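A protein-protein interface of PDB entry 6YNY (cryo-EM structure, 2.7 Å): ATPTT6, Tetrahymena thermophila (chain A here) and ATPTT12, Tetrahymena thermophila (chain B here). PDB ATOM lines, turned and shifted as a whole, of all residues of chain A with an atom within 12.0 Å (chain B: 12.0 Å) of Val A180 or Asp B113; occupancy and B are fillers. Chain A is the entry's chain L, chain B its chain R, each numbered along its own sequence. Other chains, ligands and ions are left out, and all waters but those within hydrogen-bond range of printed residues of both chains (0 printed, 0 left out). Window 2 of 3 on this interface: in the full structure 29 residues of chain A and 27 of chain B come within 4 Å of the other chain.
The backbone carbonyl oxygen (O) of Ile A184 lies within hydrogen-bond range of the guanidinium group (NH1) of Arg A189, 2.9 Å away.
The side-chain hydroxyl of Thr A179 sits at hydrogen-bond distance from the backbone carbonyl oxygen of Gln A181.
OD1 of Asp B113 lies within hydrogen-bond range of N of Leu B115.
OD2 of Asp B113 sits close to OE1 of Gln B116 (2.9 Å).
CB of Thr A179 touches OD2 of Asp B113 (3.6 Å).
Thr A179 touches Gln B116.
N of Val A180 touches OD2 of Asp B113, 3.7 Å away.
Gln A181 touches Asp B112 (NE2 to C, 3.7 Å).
N of Gln A181 touches OD2 of Asp B113, 3.6 Å away.
OE1 of Gln A181 touches CD of Pro B114, 3.7 Å away.
Asp B112 touches Pro A185 (OD1 to CA, 3.9 Å).
Glu A186 touches Gly B111.
No residue of chain B comes within 4 Å of Pro A178.
Of chain B, only Asp B113 comes within 4 Å of Val A180.
Gln A181 touches four residues of chain B.
Asn A182 touches none of the printed residues of chain B.
Printed residues of chain B within 4 Å of Pro A185: Asp B112 (3.9 Å).
Printed residues of chain B within 4 Å of Arg A189: Asp B108.
Of the printed residues of chain A, Asp B108 touches Glu A186 (2.6 Å) and Arg A189 (3.1 Å).
Gly B111 touches just these residues of chain A: Gln A181 and Glu A186.
Of chain A, only Gln A181, Pro A185 and Glu A186 come within 4 Å of Asp B112.
Asp B113 touches just these residues of chain A: Thr A179, Val A180 and Gln A181.
Of chain A, only Gln A181 (3.7 Å) comes within 4 Å of Pro B114.
Leu B115 touches none of the printed residues of chain A.
Gln B116 touches just one residue of chain A: Thr A179.
No residue of chain A comes within 4 Å of Lys B117.
The nearest residue of chain A that does not touch Asp B113 is Asn A182 (6.3 Å).
The nearest printed residue of chain B that does not touch Pro A185 is Asp B108 (5.7 Å).
Of the 14 printed residues of chain A, 6 touch a printed residue of chain B.
Along chain A the printed residues that touch a printed residue of chain B span positions 179 to 189.
Among the printed residues, 12 pairs touch across the chains.
Among the printed residues, Asp or Glu carboxylates within 4 Å of a Lys or Arg side-chain nitrogen of the other chain: Arg A189 with Asp B108 (3.2 Å).
N of Glu A186 sits at hydrogen-bond distance from OD1 of Asp B112 (3.3 Å).
NE2 of Gln A181 is in hydrogen-bond range of O of Gly B111 (3.2 Å).
NH2 of Arg A189 is in salt-bridge range of OD1 of Asp B108 (3.2 Å).
OE1 of Glu A186 sits close to OD1 of Asp B108, at 2.6 Å.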
ATOM      1  N   ARG A 176     -19.600 -20.656  10.478  1.00  0.00           N
ATOM      2  CA  ARG A 176     -18.722 -21.090   9.408  1.00  0.00           C
ATOM      3  C   ARG A 176     -18.523 -19.988   8.381  1.00  0.00           C
ATOM      4  O   ARG A 176     -19.403 -19.158   8.142  1.00  0.00           O
ATOM      5  CB  ARG A 176     -19.277 -22.346   8.745  1.00  0.00           C
ATOM      6  CG  ARG A 176     -19.179 -23.558   9.634  1.00  0.00           C
ATOM      7  CD  ARG A 176     -19.576 -24.818   8.928  1.00  0.00           C
ATOM      8  NE  ARG A 176     -19.078 -25.997   9.626  1.00  0.00           N
ATOM      9  CZ  ARG A 176     -17.878 -26.531   9.428  1.00  0.00           C
ATOM     10  NH1 ARG A 176     -17.041 -25.997   8.550  1.00  0.00           N
ATOM     11  NH2 ARG A 176     -17.511 -27.600  10.114  1.00  0.00           N
ATOM     12  N   ILE A 177     -17.342 -19.988   7.775  1.00  0.00           N
ATOM     13  CA  ILE A 177     -16.932 -18.937   6.852  1.00  0.00           C
ATOM     14  C   ILE A 177     -17.275 -19.394   5.437  1.00  0.00           C
ATOM     15  O   ILE A 177     -16.760 -20.431   4.995  1.00  0.00           O
ATOM     16  CB  ILE A 177     -15.437 -18.631   6.981  1.00  0.00           C
ATOM     17  CG1 ILE A 177     -15.071 -18.413   8.448  1.00  0.00           C
ATOM     18  CG2 ILE A 177     -15.077 -17.407   6.166  1.00  0.00           C
ATOM     19  CD1 ILE A 177     -13.613 -18.174   8.686  1.00  0.00           C
ATOM     20  N   PRO A 178     -18.123 -18.673   4.707  1.00  0.00           N
ATOM     21  CA  PRO A 178     -18.440 -19.087   3.339  1.00  0.00           C
ATOM     22  C   PRO A 178     -17.246 -18.941   2.411  1.00  0.00           C
ATOM     23  O   PRO A 178     -16.473 -17.986   2.502  1.00  0.00           O
ATOM     24  CB  PRO A 178     -19.585 -18.152   2.941  1.00  0.00           C
ATOM     25  CG  PRO A 178     -19.491 -17.011   3.839  1.00  0.00           C
ATOM     26  CD  PRO A 178     -18.898 -17.491   5.113  1.00  0.00           C
ATOM     27  N   THR A 179     -17.106 -19.910   1.515  1.00  0.00           N
ATOM     28  CA  THR A 179     -16.003 -19.965   0.575  1.00  0.00           C
ATOM     29  C   THR A 179     -16.437 -19.423  -0.780  1.00  0.00           C
ATOM     30  O   THR A 179     -17.579 -19.006  -0.981  1.00  0.00           O
ATOM     31  CB  THR A 179     -15.493 -21.399   0.442  1.00  0.00           C
ATOM     32  OG1 THR A 179     -16.533 -22.233  -0.079  1.00  0.00           O
ATOM     33  CG2 THR A 179     -15.061 -21.934   1.784  1.00  0.00           C
ATOM     34  N   VAL A 180     -15.502 -19.433  -1.729  1.00  0.00           N
ATOM     35  CA  VAL A 180     -15.820 -19.004  -3.087  1.00  0.00           C
ATOM     36  C   VAL A 180     -16.833 -19.948  -3.711  1.00  0.00           C
ATOM     37  O   VAL A 180     -17.826 -19.517  -4.308  1.00  0.00           O
ATOM     38  CB  VAL A 180     -14.540 -18.913  -3.933  1.00  0.00           C
ATOM     39  CG1 VAL A 180     -14.889 -18.601  -5.362  1.00  0.00           C
ATOM     40  CG2 VAL A 180     -13.630 -17.864  -3.375  1.00  0.00           C
ATOM     41  N   GLN A 181     -16.593 -21.251  -3.592  1.00  0.00           N
ATOM     42  CA  GLN A 181     -17.595 -22.250  -3.949  1.00  0.00           C
ATOM     43  C   GLN A 181     -18.658 -22.210  -2.860  1.00  0.00           C
ATOM     44  O   GLN A 181     -18.642 -22.973  -1.891  1.00  0.00           O
ATOM     45  CB  GLN A 181     -16.969 -23.628  -4.087  1.00  0.00           C
ATOM     46  CG  GLN A 181     -17.937 -24.710  -4.506  1.00  0.00           C
ATOM     47  CD  GLN A 181     -17.271 -26.055  -4.652  1.00  0.00           C
ATOM     48  OE1 GLN A 181     -16.248 -26.184  -5.323  1.00  0.00           O
ATOM     49  NE2 GLN A 181     -17.840 -27.065  -4.015  1.00  0.00           N
ATOM     50  N   ASN A 182     -19.597 -21.284  -3.022  1.00  0.00           N
ATOM     51  CA  ASN A 182     -20.526 -20.961  -1.952  1.00  0.00           C
ATOM     52  C   ASN A 182     -21.514 -22.099  -1.764  1.00  0.00           C
ATOM     53  O   ASN A 182     -22.537 -22.169  -2.452  1.00  0.00           O
ATOM     54  CB  ASN A 182     -21.241 -19.649  -2.257  1.00  0.00           C
ATOM     55  CG  ASN A 182     -22.034 -19.138  -1.092  1.00  0.00           C
ATOM     56  OD1 ASN A 182     -21.720 -19.413   0.063  1.00  0.00           O
ATOM     57  ND2 ASN A 182     -23.076 -18.383  -1.388  1.00  0.00           N
ATOM     58  N   ASN A 183     -21.210 -22.996  -0.833  1.00  0.00           N
ATOM     59  CA  ASN A 183     -22.045 -24.156  -0.578  1.00  0.00           C
ATOM     60  C   ASN A 183     -21.901 -24.568   0.876  1.00  0.00           C
ATOM     61  O   ASN A 183     -20.893 -24.281   1.526  1.00  0.00           O
ATOM     62  CB  ASN A 183     -21.673 -25.336  -1.481  1.00  0.00           C
ATOM     63  CG  ASN A 183     -22.219 -25.196  -2.883  1.00  0.00           C
ATOM     64  OD1 ASN A 183     -21.470 -24.984  -3.835  1.00  0.00           O
ATOM     65  ND2 ASN A 183     -23.531 -25.334  -3.020  1.00  0.00           N
ATOM     66  N   ILE A 184     -22.931 -25.229   1.377  1.00  0.00           N
ATOM     67  CA  ILE A 184     -22.851 -25.852   2.700  1.00  0.00           C
ATOM     68  C   ILE A 184     -21.867 -27.013   2.635  1.00  0.00           C
ATOM     69  O   ILE A 184     -21.784 -27.685   1.593  1.00  0.00           O
ATOM     70  CB  ILE A 184     -24.241 -26.315   3.142  1.00  0.00           C
ATOM     71  CG1 ILE A 184     -25.139 -25.100   3.353  1.00  0.00           C
ATOM     72  CG2 ILE A 184     -24.182 -27.144   4.401  1.00  0.00           C
ATOM     73  CD1 ILE A 184     -26.590 -25.417   3.402  1.00  0.00           C
ATOM     74  N   PRO A 185     -21.092 -27.279   3.685  1.00  0.00           N
ATOM     75  CA  PRO A 185     -20.128 -28.381   3.621  1.00  0.00           C
ATOM     76  C   PRO A 185     -20.788 -29.687   3.208  1.00  0.00           C
ATOM     77  O   PRO A 185     -21.892 -30.016   3.646  1.00  0.00           O
ATOM     78  CB  PRO A 185     -19.577 -28.446   5.046  1.00  0.00           C
ATOM     79  CG  PRO A 185     -19.718 -27.065   5.547  1.00  0.00           C
ATOM     80  CD  PRO A 185     -20.973 -26.533   4.947  1.00  0.00           C
ATOM     81  N   GLU A 186     -20.093 -30.431   2.348  1.00  0.00           N
ATOM     82  CA  GLU A 186     -20.635 -31.687   1.843  1.00  0.00           C
ATOM     83  C   GLU A 186     -20.947 -32.654   2.977  1.00  0.00           C
ATOM     84  O   GLU A 186     -21.957 -33.362   2.936  1.00  0.00           O
ATOM     85  CB  GLU A 186     -19.651 -32.310   0.857  1.00  0.00           C
ATOM     86  CG  GLU A 186     -20.068 -33.664   0.344  1.00  0.00           C
ATOM     87  CD  GLU A 186     -19.231 -34.118  -0.825  1.00  0.00           C
ATOM     88  OE1 GLU A 186     -19.810 -34.447  -1.880  1.00  0.00           O
ATOM     89  OE2 GLU A 186     -17.990 -34.139  -0.694  1.00  0.00           O
ATOM     90  N   ALA A 187     -20.088 -32.703   3.994  1.00  0.00           N
ATOM     91  CA  ALA A 187     -20.358 -33.558   5.142  1.00  0.00           C
ATOM     92  C   ALA A 187     -21.652 -33.159   5.834  1.00  0.00           C
ATOM     93  O   ALA A 187     -22.434 -34.019   6.250  1.00  0.00           O
ATOM     94  CB  ALA A 187     -19.193 -33.497   6.124  1.00  0.00           C
ATOM     95  N   THR A 188     -21.893 -31.856   5.966  1.00  0.00           N
ATOM     96  CA  THR A 188     -23.120 -31.390   6.597  1.00  0.00           C
ATOM     97  C   THR A 188     -24.337 -31.722   5.744  1.00  0.00           C
ATOM     98  O   THR A 188     -25.396 -32.073   6.275  1.00  0.00           O
ATOM     99  CB  THR A 188     -23.023 -29.887   6.855  1.00  0.00           C
ATOM    100  OG1 THR A 188     -21.964 -29.632   7.784  1.00  0.00           O
ATOM    101  CG2 THR A 188     -24.313 -29.340   7.413  1.00  0.00           C
ATOM    102  N   ARG A 189     -24.206 -31.618   4.422  1.00  0.00           N
ATOM    103  CA  ARG A 189     -25.305 -31.991   3.541  1.00  0.00           C
ATOM    104  C   ARG A 189     -25.559 -33.492   3.579  1.00  0.00           C
ATOM    105  O   ARG A 189     -26.713 -33.933   3.554  1.00  0.00           O
ATOM    106  CB  ARG A 189     -25.013 -31.539   2.113  1.00  0.00           C
ATOM    107  CG  ARG A 189     -25.179 -30.056   1.884  1.00  0.00           C
ATOM    108  CD  ARG A 189     -24.074 -29.496   1.021  1.00  0.00           C
ATOM    109  NE  ARG A 189     -24.190 -29.868  -0.381  1.00  0.00           N
ATOM    110  CZ  ARG A 189     -23.226 -29.677  -1.275  1.00  0.00           C
ATOM    111  NH1 ARG A 189     -22.078 -29.133  -0.905  1.00  0.00           N
ATOM    112  NH2 ARG A 189     -23.408 -30.035  -2.535  1.00  0.00           N
ATOM    113  N   ASP B 108     -23.609 -35.543  -3.149  1.00  0.00           N
ATOM    114  CA  ASP B 108     -23.769 -34.325  -3.915  1.00  0.00           C
ATOM    115  C   ASP B 108     -22.574 -34.113  -4.829  1.00  0.00           C
ATOM    116  O   ASP B 108     -21.493 -34.665  -4.601  1.00  0.00           O
ATOM    117  CB  ASP B 108     -23.927 -33.112  -2.993  1.00  0.00           C
ATOM    118  CG  ASP B 108     -22.887 -33.071  -1.900  1.00  0.00           C
ATOM    119  OD1 ASP B 108     -21.716 -32.773  -2.210  1.00  0.00           O
ATOM    120  OD2 ASP B 108     -23.244 -33.334  -0.731  1.00  0.00           O
ATOM    121  N   PRO B 109     -22.735 -33.328  -5.885  1.00  0.00           N
ATOM    122  CA  PRO B 109     -21.653 -33.166  -6.855  1.00  0.00           C
ATOM    123  C   PRO B 109     -20.623 -32.146  -6.395  1.00  0.00           C
ATOM    124  O   PRO B 109     -20.889 -31.271  -5.571  1.00  0.00           O
ATOM    125  CB  PRO B 109     -22.386 -32.689  -8.108  1.00  0.00           C
ATOM    126  CG  PRO B 109     -23.563 -31.961  -7.588  1.00  0.00           C
ATOM    127  CD  PRO B 109     -23.959 -32.624  -6.306  1.00  0.00           C
ATOM    128  N   ALA B 110     -19.424 -32.279  -6.951  1.00  0.00           N
ATOM    129  CA  ALA B 110     -18.319 -31.335  -6.860  1.00  0.00           C
ATOM    130  C   ALA B 110     -17.605 -31.375  -5.513  1.00  0.00           C
ATOM    131  O   ALA B 110     -16.551 -30.750  -5.380  1.00  0.00           O
ATOM    132  CB  ALA B 110     -18.758 -29.884  -7.122  1.00  0.00           C
ATOM    133  N   GLY B 111     -18.115 -32.094  -4.522  1.00  0.00           N
ATOM    134  CA  GLY B 111     -17.432 -32.152  -3.242  1.00  0.00           C
ATOM    135  C   GLY B 111     -17.268 -30.776  -2.632  1.00  0.00           C
ATOM    136  O   GLY B 111     -18.165 -29.928  -2.698  1.00  0.00           O
ATOM    137  N   ASP B 112     -16.107 -30.544  -2.031  1.00  0.00           N
ATOM    138  CA  ASP B 112     -15.804 -29.283  -1.375  1.00  0.00           C
ATOM    139  C   ASP B 112     -14.897 -28.419  -2.243  1.00  0.00           C
ATOM    140  O   ASP B 112     -14.381 -28.846  -3.278  1.00  0.00           O
ATOM    141  CB  ASP B 112     -15.156 -29.529  -0.011  1.00  0.00           C
ATOM    142  CG  ASP B 112     -16.169 -29.882   1.059  1.00  0.00           C
ATOM    143  OD1 ASP B 112     -17.255 -29.265   1.078  1.00  0.00           O
ATOM    144  OD2 ASP B 112     -15.882 -30.776   1.879  1.00  0.00           O
ATOM    145  N   ASP B 113     -14.702 -27.188  -1.793  1.00  0.00           N
ATOM    146  CA  ASP B 113     -13.931 -26.205  -2.537  1.00  0.00           C
ATOM    147  C   ASP B 113     -12.476 -26.650  -2.646  1.00  0.00           C
ATOM    148  O   ASP B 113     -11.806 -26.795  -1.613  1.00  0.00           O
ATOM    149  CB  ASP B 113     -14.024 -24.845  -1.856  1.00  0.00           C
ATOM    150  CG  ASP B 113     -13.408 -23.735  -2.681  1.00  0.00           C
ATOM    151  OD1 ASP B 113     -12.833 -24.030  -3.748  1.00  0.00           O
ATOM    152  OD2 ASP B 113     -13.508 -22.562  -2.264  1.00  0.00           O
ATOM    153  N   PRO B 114     -11.952 -26.878  -3.852  1.00  0.00           N
ATOM    154  CA  PRO B 114     -10.537 -27.263  -3.962  1.00  0.00           C
ATOM    155  C   PRO B 114      -9.576 -26.170  -3.540  1.00  0.00           C
ATOM    156  O   PRO B 114      -8.488 -26.481  -3.043  1.00  0.00           O
ATOM    157  CB  PRO B 114     -10.380 -27.597  -5.450  1.00  0.00           C
ATOM    158  CG  PRO B 114     -11.745 -27.857  -5.937  1.00  0.00           C
ATOM    159  CD  PRO B 114     -12.641 -26.976  -5.147  1.00  0.00           C
ATOM    160  N   LEU B 115      -9.935 -24.901  -3.725  1.00  0.00           N
ATOM    161  CA  LEU B 115      -9.029 -23.814  -3.390  1.00  0.00           C
ATOM    162  C   LEU B 115      -8.790 -23.686  -1.895  1.00  0.00           C
ATOM    163  O   LEU B 115      -7.870 -22.966  -1.492  1.00  0.00           O
ATOM    164  CB  LEU B 115      -9.578 -22.502  -3.938  1.00  0.00           C
ATOM    165  CG  LEU B 115      -9.778 -22.475  -5.450  1.00  0.00           C
ATOM    166  CD1 LEU B 115     -10.398 -21.169  -5.860  1.00  0.00           C
ATOM    167  CD2 LEU B 115      -8.462 -22.683  -6.166  1.00  0.00           C
ATOM    168  N   GLN B 116      -9.587 -24.354  -1.069  1.00  0.00           N
ATOM    169  CA  GLN B 116      -9.368 -24.392   0.367  1.00  0.00           C
ATOM    170  C   GLN B 116      -8.537 -25.591   0.791  1.00  0.00           C
ATOM    171  O   GLN B 116      -8.384 -25.834   1.992  1.00  0.00           O
ATOM    172  CB  GLN B 116     -10.710 -24.402   1.099  1.00  0.00           C
ATOM    173  CG  GLN B 116     -11.034 -23.108   1.812  1.00  0.00           C
ATOM    174  CD  GLN B 116     -11.087 -21.922   0.879  1.00  0.00           C
ATOM    175  OE1 GLN B 116     -11.990 -21.808   0.052  1.00  0.00           O
ATOM    176  NE2 GLN B 116     -10.110 -21.029   1.002  1.00  0.00           N
ATOM    177  N   LYS B 117      -7.996 -26.340  -0.163  1.00  0.00           N
ATOM    178  CA  LYS B 117      -7.164 -27.497   0.111  1.00  0.00           C
ATOM    179  C   LYS B 117      -5.705 -27.175  -0.180  1.00  0.00           C
ATOM    180  O   LYS B 117      -5.381 -26.191  -0.849  1.00  0.00           O
ATOM    181  CB  LYS B 117      -7.616 -28.697  -0.721  1.00  0.00           C
ATOM    182  CG  LYS B 117      -9.023 -29.137  -0.403  1.00  0.00           C
ATOM    183  CD  LYS B 117      -9.402 -30.384  -1.159  1.00  0.00           C
ATOM    184  CE  LYS B 117     -10.793 -30.844  -0.777  1.00  0.00           C
ATOM    185  NZ  LYS B 117     -11.100 -32.195  -1.309  1.00  0.00           N
ATOM    186  N   THR B 118      -4.826 -28.029   0.332  1.00  0.00           N
ATOM    187  CA  THR B 118      -3.397 -27.817   0.168  1.00  0.00           C
ATOM    188  C   THR B 118      -3.019 -27.852  -1.305  1.00  0.00           C
ATOM    189  O   THR B 118      -3.417 -28.757  -2.043  1.00  0.00           O
ATOM    190  CB  THR B 118      -2.620 -28.878   0.943  1.00  0.00           C
ATOM    191  OG1 THR B 118      -3.031 -28.869   2.314  1.00  0.00           O
ATOM    192  CG2 THR B 118      -1.138 -28.610   0.865  1.00  0.00           C
ATOM    193  N   LYS B 119      -2.244 -26.860  -1.729  1.00  0.00           N
ATOM    194  CA  LYS B 119      -1.840 -26.754  -3.119  1.00  0.00           C
ATOM    195  C   LYS B 119      -0.620 -27.622  -3.393  1.00  0.00           C
ATOM    196  O   LYS B 119       0.202 -27.877  -2.509  1.00  0.00           O
ATOM    197  CB  LYS B 119      -1.512 -25.307  -3.478  1.00  0.00           C
ATOM    198  CG  LYS B 119      -2.490 -24.277  -2.955  1.00  0.00           C
ATOM    199  CD  LYS B 119      -3.832 -24.375  -3.629  1.00  0.00           C
ATOM    200  CE  LYS B 119      -4.763 -23.290  -3.135  1.00  0.00           C
ATOM    201  NZ  LYS B 119      -4.249 -21.935  -3.448  1.00  0.00           N
ATOM    202  N   ASP B 120      -0.506 -28.071  -4.641  1.00  0.00           N
ATOM    203  CA  ASP B 120       0.685 -28.788  -5.070  1.00  0.00           C
ATOM    204  C   ASP B 120       1.838 -27.839  -5.360  1.00  0.00           C
ATOM    205  O   ASP B 120       2.999 -28.193  -5.136  1.00  0.00           O
ATOM    206  CB  ASP B 120       0.375 -29.629  -6.306  1.00  0.00           C
ATOM    207  CG  ASP B 120      -0.319 -30.932  -5.967  1.00  0.00           C
ATOM    208  OD1 ASP B 120      -0.538 -31.200  -4.767  1.00  0.00           O
ATOM    209  OD2 ASP B 120      -0.639 -31.695  -6.902  1.00  0.00           O
